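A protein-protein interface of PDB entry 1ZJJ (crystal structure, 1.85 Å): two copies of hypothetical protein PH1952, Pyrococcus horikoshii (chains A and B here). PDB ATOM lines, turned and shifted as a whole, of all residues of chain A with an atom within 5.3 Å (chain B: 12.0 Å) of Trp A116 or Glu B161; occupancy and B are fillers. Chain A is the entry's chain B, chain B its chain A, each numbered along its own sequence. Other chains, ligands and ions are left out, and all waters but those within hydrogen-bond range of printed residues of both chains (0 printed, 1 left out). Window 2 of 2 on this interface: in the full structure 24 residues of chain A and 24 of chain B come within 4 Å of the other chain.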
ATOM      1  N   VAL A 106      13.259  12.392  10.523  1.00  0.00           N
ATOM      2  CA  VAL A 106      14.203  11.385  10.054  1.00  0.00           C
ATOM      3  C   VAL A 106      13.582  10.797   8.787  1.00  0.00           C
ATOM      4  O   VAL A 106      12.501  10.201   8.836  1.00  0.00           O
ATOM      5  CB  VAL A 106      14.397  10.251  11.091  1.00  0.00           C
ATOM      6  CG1 VAL A 106      15.308   9.165  10.513  1.00  0.00           C
ATOM      7  CG2 VAL A 106      14.996  10.813  12.373  1.00  0.00           C
ATOM      8  N   GLU A 110      17.690   8.276   5.728  1.00  0.00           N
ATOM      9  CA  GLU A 110      18.474   8.386   6.949  1.00  0.00           C
ATOM     10  C   GLU A 110      18.176   7.153   7.801  1.00  0.00           C
ATOM     11  O   GLU A 110      19.068   6.604   8.444  1.00  0.00           O
ATOM     12  CB  GLU A 110      18.108   9.676   7.692  1.00  0.00           C
ATOM     13  CG  GLU A 110      18.363  10.925   6.858  1.00  0.00           C
ATOM     14  CD  GLU A 110      17.937  12.204   7.554  1.00  0.00           C
ATOM     15  OE1 GLU A 110      16.817  12.242   8.107  1.00  0.00           O
ATOM     16  OE2 GLU A 110      18.720  13.176   7.532  1.00  0.00           O
ATOM     17  N   ALA A 111      16.920   6.707   7.774  1.00  0.00           N
ATOM     18  CA  ALA A 111      16.507   5.525   8.526  1.00  0.00           C
ATOM     19  C   ALA A 111      17.280   4.299   8.040  1.00  0.00           C
ATOM     20  O   ALA A 111      17.723   3.471   8.842  1.00  0.00           O
ATOM     21  CB  ALA A 111      15.002   5.289   8.364  1.00  0.00           C
ATOM     22  N   GLY A 114      20.404   3.775   9.563  1.00  0.00           N
ATOM     23  CA  GLY A 114      20.347   3.475  10.985  1.00  0.00           C
ATOM     24  C   GLY A 114      19.799   4.554  11.903  1.00  0.00           C
ATOM     25  O   GLY A 114      19.753   4.359  13.121  1.00  0.00           O
ATOM     26  N   SER A 115      19.381   5.681  11.331  1.00  0.00           N
ATOM     27  CA  SER A 115      18.856   6.802  12.116  1.00  0.00           C
ATOM     28  C   SER A 115      17.532   6.533  12.826  1.00  0.00           C
ATOM     29  O   SER A 115      17.082   7.352  13.627  1.00  0.00           O
ATOM     30  CB  SER A 115      18.707   8.043  11.234  1.00  0.00           C
ATOM     31  OG  SER A 115      19.970   8.478  10.758  1.00  0.00           O
ATOM     32  N   TRP A 116      16.896   5.405  12.528  1.00  0.00           N
ATOM     33  CA  TRP A 116      15.640   5.072  13.200  1.00  0.00           C
ATOM     34  C   TRP A 116      15.929   4.968  14.699  1.00  0.00           C
ATOM     35  O   TRP A 116      15.043   5.174  15.536  1.00  0.00           O
ATOM     36  CB  TRP A 116      15.093   3.733  12.711  1.00  0.00           C
ATOM     37  CG  TRP A 116      16.069   2.591  12.824  1.00  0.00           C
ATOM     38  CD1 TRP A 116      16.920   2.147  11.852  1.00  0.00           C
ATOM     39  CD2 TRP A 116      16.272   1.750  13.968  1.00  0.00           C
ATOM     40  NE1 TRP A 116      17.638   1.070  12.331  1.00  0.00           N
ATOM     41  CE2 TRP A 116      17.255   0.806  13.626  1.00  0.00           C
ATOM     42  CE3 TRP A 116      15.707   1.702  15.255  1.00  0.00           C
ATOM     43  CZ2 TRP A 116      17.694  -0.170  14.503  1.00  0.00           C
ATOM     44  CZ3 TRP A 116      16.144   0.727  16.142  1.00  0.00           C
ATOM     45  CH2 TRP A 116      17.135  -0.204  15.752  1.00  0.00           C
ATOM     46  N   LYS A 117      17.191   4.650  15.008  1.00  0.00           N
ATOM     47  CA  LYS A 117      17.687   4.497  16.375  1.00  0.00           C
ATOM     48  C   LYS A 117      17.577   5.807  17.154  1.00  0.00           C
ATOM     49  O   LYS A 117      17.470   5.799  18.370  1.00  0.00           O
ATOM     50  CB  LYS A 117      19.155   4.041  16.341  1.00  0.00           C
ATOM     51  CG  LYS A 117      19.475   2.812  17.186  1.00  0.00           C
ATOM     52  CD  LYS A 117      19.031   2.980  18.619  1.00  0.00           C
ATOM     53  CE  LYS A 117      19.622   1.873  19.455  1.00  0.00           C
ATOM     54  NZ  LYS A 117      18.844   1.621  20.675  1.00  0.00           N
ATOM     55  N   GLU A 118      17.616   6.932  16.447  1.00  0.00           N
ATOM     56  CA  GLU A 118      17.522   8.233  17.106  1.00  0.00           C
ATOM     57  C   GLU A 118      16.117   8.846  17.115  1.00  0.00           C
ATOM     58  O   GLU A 118      15.915   9.942  17.637  1.00  0.00           O
ATOM     59  CB  GLU A 118      18.513   9.223  16.472  1.00  0.00           C
ATOM     60  CG  GLU A 118      19.978   8.910  16.755  1.00  0.00           C
ATOM     61  CD  GLU A 118      20.519   7.718  15.974  1.00  0.00           C
ATOM     62  OE1 GLU A 118      20.544   7.762  14.729  1.00  0.00           O
ATOM     63  OE2 GLU A 118      20.926   6.720  16.603  1.00  0.00           O
ATOM     64  N   VAL A 119      15.154   8.149  16.527  1.00  0.00           N
ATOM     65  CA  VAL A 119      13.776   8.642  16.479  1.00  0.00           C
ATOM     66  C   VAL A 119      13.121   8.656  17.858  1.00  0.00           C
ATOM     67  O   VAL A 119      13.179   7.663  18.582  1.00  0.00           O
ATOM     68  CB  VAL A 119      12.906   7.769  15.547  1.00  0.00           C
ATOM     69  CG1 VAL A 119      11.423   8.121  15.726  1.00  0.00           C
ATOM     70  CG2 VAL A 119      13.333   7.968  14.107  1.00  0.00           C
ATOM     71  N   LYS A 136       8.633  -1.451   9.028  1.00  0.00           N
ATOM     72  CA  LYS A 136       9.813  -1.983   9.693  1.00  0.00           C
ATOM     73  C   LYS A 136      10.496  -0.933  10.576  1.00  0.00           C
ATOM     74  O   LYS A 136      10.660  -1.136  11.776  1.00  0.00           O
ATOM     75  CB  LYS A 136      10.801  -2.510   8.649  1.00  0.00           C
ATOM     76  CG  LYS A 136      12.087  -3.080   9.239  1.00  0.00           C
ATOM     77  CD  LYS A 136      13.096  -3.435   8.152  1.00  0.00           C
ATOM     78  CE  LYS A 136      13.554  -2.210   7.365  1.00  0.00           C
ATOM     79  NZ  LYS A 136      14.626  -2.558   6.383  1.00  0.00           N
ATOM     80  N   TYR A 137      10.895   0.189   9.987  1.00  0.00           N
ATOM     81  CA  TYR A 137      11.557   1.232  10.764  1.00  0.00           C
ATOM     82  C   TYR A 137      10.660   1.817  11.845  1.00  0.00           C
ATOM     83  O   TYR A 137      11.130   2.147  12.935  1.00  0.00           O
ATOM     84  CB  TYR A 137      12.085   2.330   9.838  1.00  0.00           C
ATOM     85  CG  TYR A 137      13.281   1.857   9.053  1.00  0.00           C
ATOM     86  CD1 TYR A 137      14.412   1.384   9.713  1.00  0.00           C
ATOM     87  CD2 TYR A 137      13.261   1.808   7.660  1.00  0.00           C
ATOM     88  CE1 TYR A 137      15.494   0.861   9.008  1.00  0.00           C
ATOM     89  CE2 TYR A 137      14.342   1.286   6.938  1.00  0.00           C
ATOM     90  CZ  TYR A 137      15.452   0.815   7.625  1.00  0.00           C
ATOM     91  OH  TYR A 137      16.527   0.289   6.942  1.00  0.00           O
ATOM     92  N   LEU A 140      10.771  -0.732  14.622  1.00  0.00           N
ATOM     93  CA  LEU A 140      12.064  -0.704  15.297  1.00  0.00           C
ATOM     94  C   LEU A 140      12.150   0.516  16.205  1.00  0.00           C
ATOM     95  O   LEU A 140      12.582   0.413  17.350  1.00  0.00           O
ATOM     96  CB  LEU A 140      13.204  -0.680  14.271  1.00  0.00           C
ATOM     97  CG  LEU A 140      13.444  -1.990  13.508  1.00  0.00           C
ATOM     98  CD1 LEU A 140      14.465  -1.786  12.407  1.00  0.00           C
ATOM     99  CD2 LEU A 140      13.914  -3.058  14.480  1.00  0.00           C
ATOM    100  N   ALA A 141      11.714   1.663  15.699  1.00  0.00           N
ATOM    101  CA  ALA A 141      11.754   2.902  16.474  1.00  0.00           C
ATOM    102  C   ALA A 141      10.830   2.852  17.692  1.00  0.00           C
ATOM    103  O   ALA A 141      11.245   3.156  18.806  1.00  0.00           O
ATOM    104  CB  ALA A 141      11.390   4.077  15.581  1.00  0.00           C
ATOM    105  N   ASN A 144      12.102   0.823  20.278  1.00  0.00           N
ATOM    106  CA  ASN A 144      13.270   1.438  20.894  1.00  0.00           C
ATOM    107  C   ASN A 144      12.866   2.556  21.860  1.00  0.00           C
ATOM    108  O   ASN A 144      13.716   3.281  22.391  1.00  0.00           O
ATOM    109  CB  ASN A 144      14.197   1.989  19.818  1.00  0.00           C
ATOM    110  CG  ASN A 144      15.540   2.417  20.375  1.00  0.00           C
ATOM    111  OD1 ASN A 144      16.179   1.672  21.118  1.00  0.00           O
ATOM    112  ND2 ASN A 144      15.984   3.610  20.002  1.00  0.00           N
ATOM    113  N   GLY B  15      19.154 -18.368  14.025  1.00  0.00           N
ATOM    114  CA  GLY B  15      19.588 -17.481  12.974  1.00  0.00           C
ATOM    115  C   GLY B  15      20.424 -18.187  11.927  1.00  0.00           C
ATOM    116  O   GLY B  15      19.879 -18.781  10.995  1.00  0.00           O
ATOM    117  N   ASN B  16      21.741 -18.163  12.101  1.00  0.00           N
ATOM    118  CA  ASN B  16      22.632 -18.741  11.112  1.00  0.00           C
ATOM    119  C   ASN B  16      23.482 -19.943  11.535  1.00  0.00           C
ATOM    120  O   ASN B  16      24.237 -20.476  10.720  1.00  0.00           O
ATOM    121  CB  ASN B  16      23.549 -17.630  10.579  1.00  0.00           C
ATOM    122  CG  ASN B  16      22.993 -16.228  10.837  1.00  0.00           C
ATOM    123  OD1 ASN B  16      23.214 -15.640  11.903  1.00  0.00           O
ATOM    124  ND2 ASN B  16      22.247 -15.694   9.865  1.00  0.00           N
ATOM    125  N   THR B 156       5.439 -10.951  15.044  1.00  0.00           N
ATOM    126  CA  THR B 156       6.770 -10.498  14.647  1.00  0.00           C
ATOM    127  C   THR B 156       7.707 -11.674  14.391  1.00  0.00           C
ATOM    128  O   THR B 156       7.367 -12.825  14.647  1.00  0.00           O
ATOM    129  CB  THR B 156       7.438  -9.689  15.770  1.00  0.00           C
ATOM    130  OG1 THR B 156       7.702 -10.567  16.872  1.00  0.00           O
ATOM    131  CG2 THR B 156       6.544  -8.552  16.247  1.00  0.00           C
ATOM    132  N   LEU B 157       8.896 -11.360  13.889  1.00  0.00           N
ATOM    133  CA  LEU B 157       9.940 -12.355  13.660  1.00  0.00           C
ATOM    134  C   LEU B 157      11.277 -11.637  13.730  1.00  0.00           C
ATOM    135  O   LEU B 157      11.355 -10.437  13.470  1.00  0.00           O
ATOM    136  CB  LEU B 157       9.798 -13.069  12.305  1.00  0.00           C
ATOM    137  CG  LEU B 157       9.743 -12.396  10.928  1.00  0.00           C
ATOM    138  CD1 LEU B 157      10.709 -11.237  10.795  1.00  0.00           C
ATOM    139  CD2 LEU B 157      10.058 -13.473   9.899  1.00  0.00           C
ATOM    140  N   PRO B 158      12.348 -12.358  14.097  1.00  0.00           N
ATOM    141  CA  PRO B 158      13.679 -11.757  14.197  1.00  0.00           C
ATOM    142  C   PRO B 158      14.198 -11.194  12.882  1.00  0.00           C
ATOM    143  O   PRO B 158      14.093 -11.834  11.835  1.00  0.00           O
ATOM    144  CB  PRO B 158      14.540 -12.912  14.704  1.00  0.00           C
ATOM    145  CG  PRO B 158      13.582 -13.702  15.521  1.00  0.00           C
ATOM    146  CD  PRO B 158      12.359 -13.728  14.638  1.00  0.00           C
ATOM    147  N   GLY B 159      14.754  -9.990  12.955  1.00  0.00           N
ATOM    148  CA  GLY B 159      15.310  -9.335  11.788  1.00  0.00           C
ATOM    149  C   GLY B 159      16.740  -8.938  12.096  1.00  0.00           C
ATOM    150  O   GLY B 159      17.145  -8.954  13.256  1.00  0.00           O
ATOM    151  N   GLU B 160      17.510  -8.593  11.072  1.00  0.00           N
ATOM    152  CA  GLU B 160      18.900  -8.200  11.279  1.00  0.00           C
ATOM    153  C   GLU B 160      19.031  -7.139  12.366  1.00  0.00           C
ATOM    154  O   GLU B 160      19.798  -7.299  13.319  1.00  0.00           O
ATOM    155  CB  GLU B 160      19.494  -7.657   9.976  1.00  0.00           C
ATOM    156  CG  GLU B 160      20.679  -6.710  10.171  1.00  0.00           C
ATOM    157  CD  GLU B 160      21.960  -7.413  10.589  1.00  0.00           C
ATOM    158  OE1 GLU B 160      21.917  -8.247  11.516  1.00  0.00           O
ATOM    159  OE2 GLU B 160      23.019  -7.118   9.993  1.00  0.00           O
ATOM    160  N   GLU B 161      18.262  -6.064  12.222  1.00  0.00           N
ATOM    161  CA  GLU B 161      18.307  -4.945  13.153  1.00  0.00           C
ATOM    162  C   GLU B 161      17.429  -5.043  14.398  1.00  0.00           C
ATOM    163  O   GLU B 161      17.387  -4.112  15.200  1.00  0.00           O
ATOM    164  CB  GLU B 161      17.989  -3.655  12.397  1.00  0.00           C
ATOM    165  CG  GLU B 161      18.971  -3.357  11.278  1.00  0.00           C
ATOM    166  CD  GLU B 161      18.732  -2.009  10.628  1.00  0.00           C
ATOM    167  OE1 GLU B 161      17.930  -1.934   9.676  1.00  0.00           O
ATOM    168  OE2 GLU B 161      19.346  -1.017  11.080  1.00  0.00           O
ATOM    169  N   GLY B 162      16.739  -6.162  14.571  1.00  0.00           N
ATOM    170  CA  GLY B 162      15.894  -6.309  15.742  1.00  0.00           C
ATOM    171  C   GLY B 162      14.621  -7.089  15.474  1.00  0.00           C
ATOM    172  O   GLY B 162      14.635  -8.084  14.749  1.00  0.00           O
ATOM    173  N   ILE B 163      13.519  -6.636  16.063  1.00  0.00           N
ATOM    174  CA  ILE B 163      12.235  -7.298  15.888  1.00  0.00           C
ATOM    175  C   ILE B 163      11.454  -6.632  14.758  1.00  0.00           C
ATOM    176  O   ILE B 163      11.128  -5.448  14.834  1.00  0.00           O
ATOM    177  CB  ILE B 163      11.409  -7.243  17.185  1.00  0.00           C
ATOM    178  CG1 ILE B 163      12.220  -7.829  18.342  1.00  0.00           C
ATOM    179  CG2 ILE B 163      10.125  -8.032  17.015  1.00  0.00           C
ATOM    180  CD1 ILE B 163      12.594  -9.287  18.157  1.00  0.00           C
ATOM    181  N   TYR B 164      11.159  -7.407  13.713  1.00  0.00           N
ATOM    182  CA  TYR B 164      10.436  -6.917  12.537  1.00  0.00           C
ATOM    183  C   TYR B 164       8.974  -7.357  12.550  1.00  0.00           C
ATOM    184  O   TYR B 164       8.608  -8.299  13.247  1.00  0.00           O
ATOM    185  CB  TYR B 164      11.075  -7.467  11.256  1.00  0.00           C
ATOM    186  CG  TYR B 164      12.457  -6.957  10.908  1.00  0.00           C
ATOM    187  CD1 TYR B 164      13.225  -6.240  11.828  1.00  0.00           C
ATOM    188  CD2 TYR B 164      13.005  -7.211   9.650  1.00  0.00           C
ATOM    189  CE1 TYR B 164      14.506  -5.790  11.503  1.00  0.00           C
ATOM    190  CE2 TYR B 164      14.284  -6.767   9.313  1.00  0.00           C
ATOM    191  CZ  TYR B 164      15.027  -6.056  10.246  1.00  0.00           C
ATOM    192  OH  TYR B 164      16.289  -5.607   9.918  1.00  0.00           O
ATOM    193  N   PRO B 165       8.118  -6.674  11.773  1.00  0.00           N
ATOM    194  CA  PRO B 165       6.697  -7.044  11.721  1.00  0.00           C
ATOM    195  C   PRO B 165       6.543  -8.410  11.042  1.00  0.00           C
ATOM    196  O   PRO B 165       7.200  -8.686  10.038  1.00  0.00           O
ATOM    197  CB  PRO B 165       6.077  -5.929  10.880  1.00  0.00           C
ATOM    198  CG  PRO B 165       6.974  -4.764  11.132  1.00  0.00           C
ATOM    199  CD  PRO B 165       8.346  -5.388  11.095  1.00  0.00           C
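No residue of chain B comes within 4 Å of Ser A115. No residue of chain B comes within 4 Å of Lys A117. No residue of chain B comes within 4 Å of Val A119. Of the printed residues of chain B, Lys A136 touches Tyr B164 and Pro B165. Tyr A137 touches just one residue of chain B: Glu B161 (3.8 Å). Printed residues of chain B within 4 Å of Leu A140: Glu B161 (3.7 Å) and Ile B163 (3.7 Å). Asn A144 touches none of the printed residues of chain B. Thr B156 touches none of the printed residues of chain A. Of chain A, only Trp A116, Tyr A137 and Leu A140 come within 4 Å of Glu B161. Gly B162 touches none of the printed residues of chain A. The nearest residue of chain B that does not touch Trp A116 is Gly B162 (6.1 Å).
Among the printed residues, pairs that only touch across the chains: Leu A140 with Ile B163 (3.7 Å), Leu A140 with Glu B161 (3.7 Å), Lys A136 with Tyr B164 (3.7 Å), Tyr A137 with Glu B161 (3.8 Å) and Lys A136 with Pro B165 (3.96 Å).
No position is printed for both chains. Of the 6 pairs that touch across the chains among the printed residues, none has its exchanged pair printed and touching as well.
Hydrophobic or aromatic side chains of chain B within 4 Å of the printed part of chain A: Tyr B164 and Pro B165. Among the printed residues, 6 pairs touch across the chains. Among the printed residues, no Asp or Glu carboxylate lies within 4 Å of a Lys or Arg side-chain nitrogen of the other chain.
OE2 of Glu B161 lies within hydrogen-bond range of NE1 of Trp A116, 3.0 Å away.
The backbone carbonyl oxygen (O) of Leu B157 lies within hydrogen-bond range of the backbone NH (N) of Tyr B164 (3.0 Å). N of Glu B160 lies within hydrogen-bond range of OH of Tyr B164, at 3.4 Å. The side-chain hydroxyl (OH) of Tyr B164 is in hydrogen-bond range of the backbone NH (N) of Glu B161 (3.1 Å). The side-chain amino group (NZ) of Lys A136 is in hydrogen-bond range of the side-chain hydroxyl (OH) of Tyr A137, at 3.5 Å.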
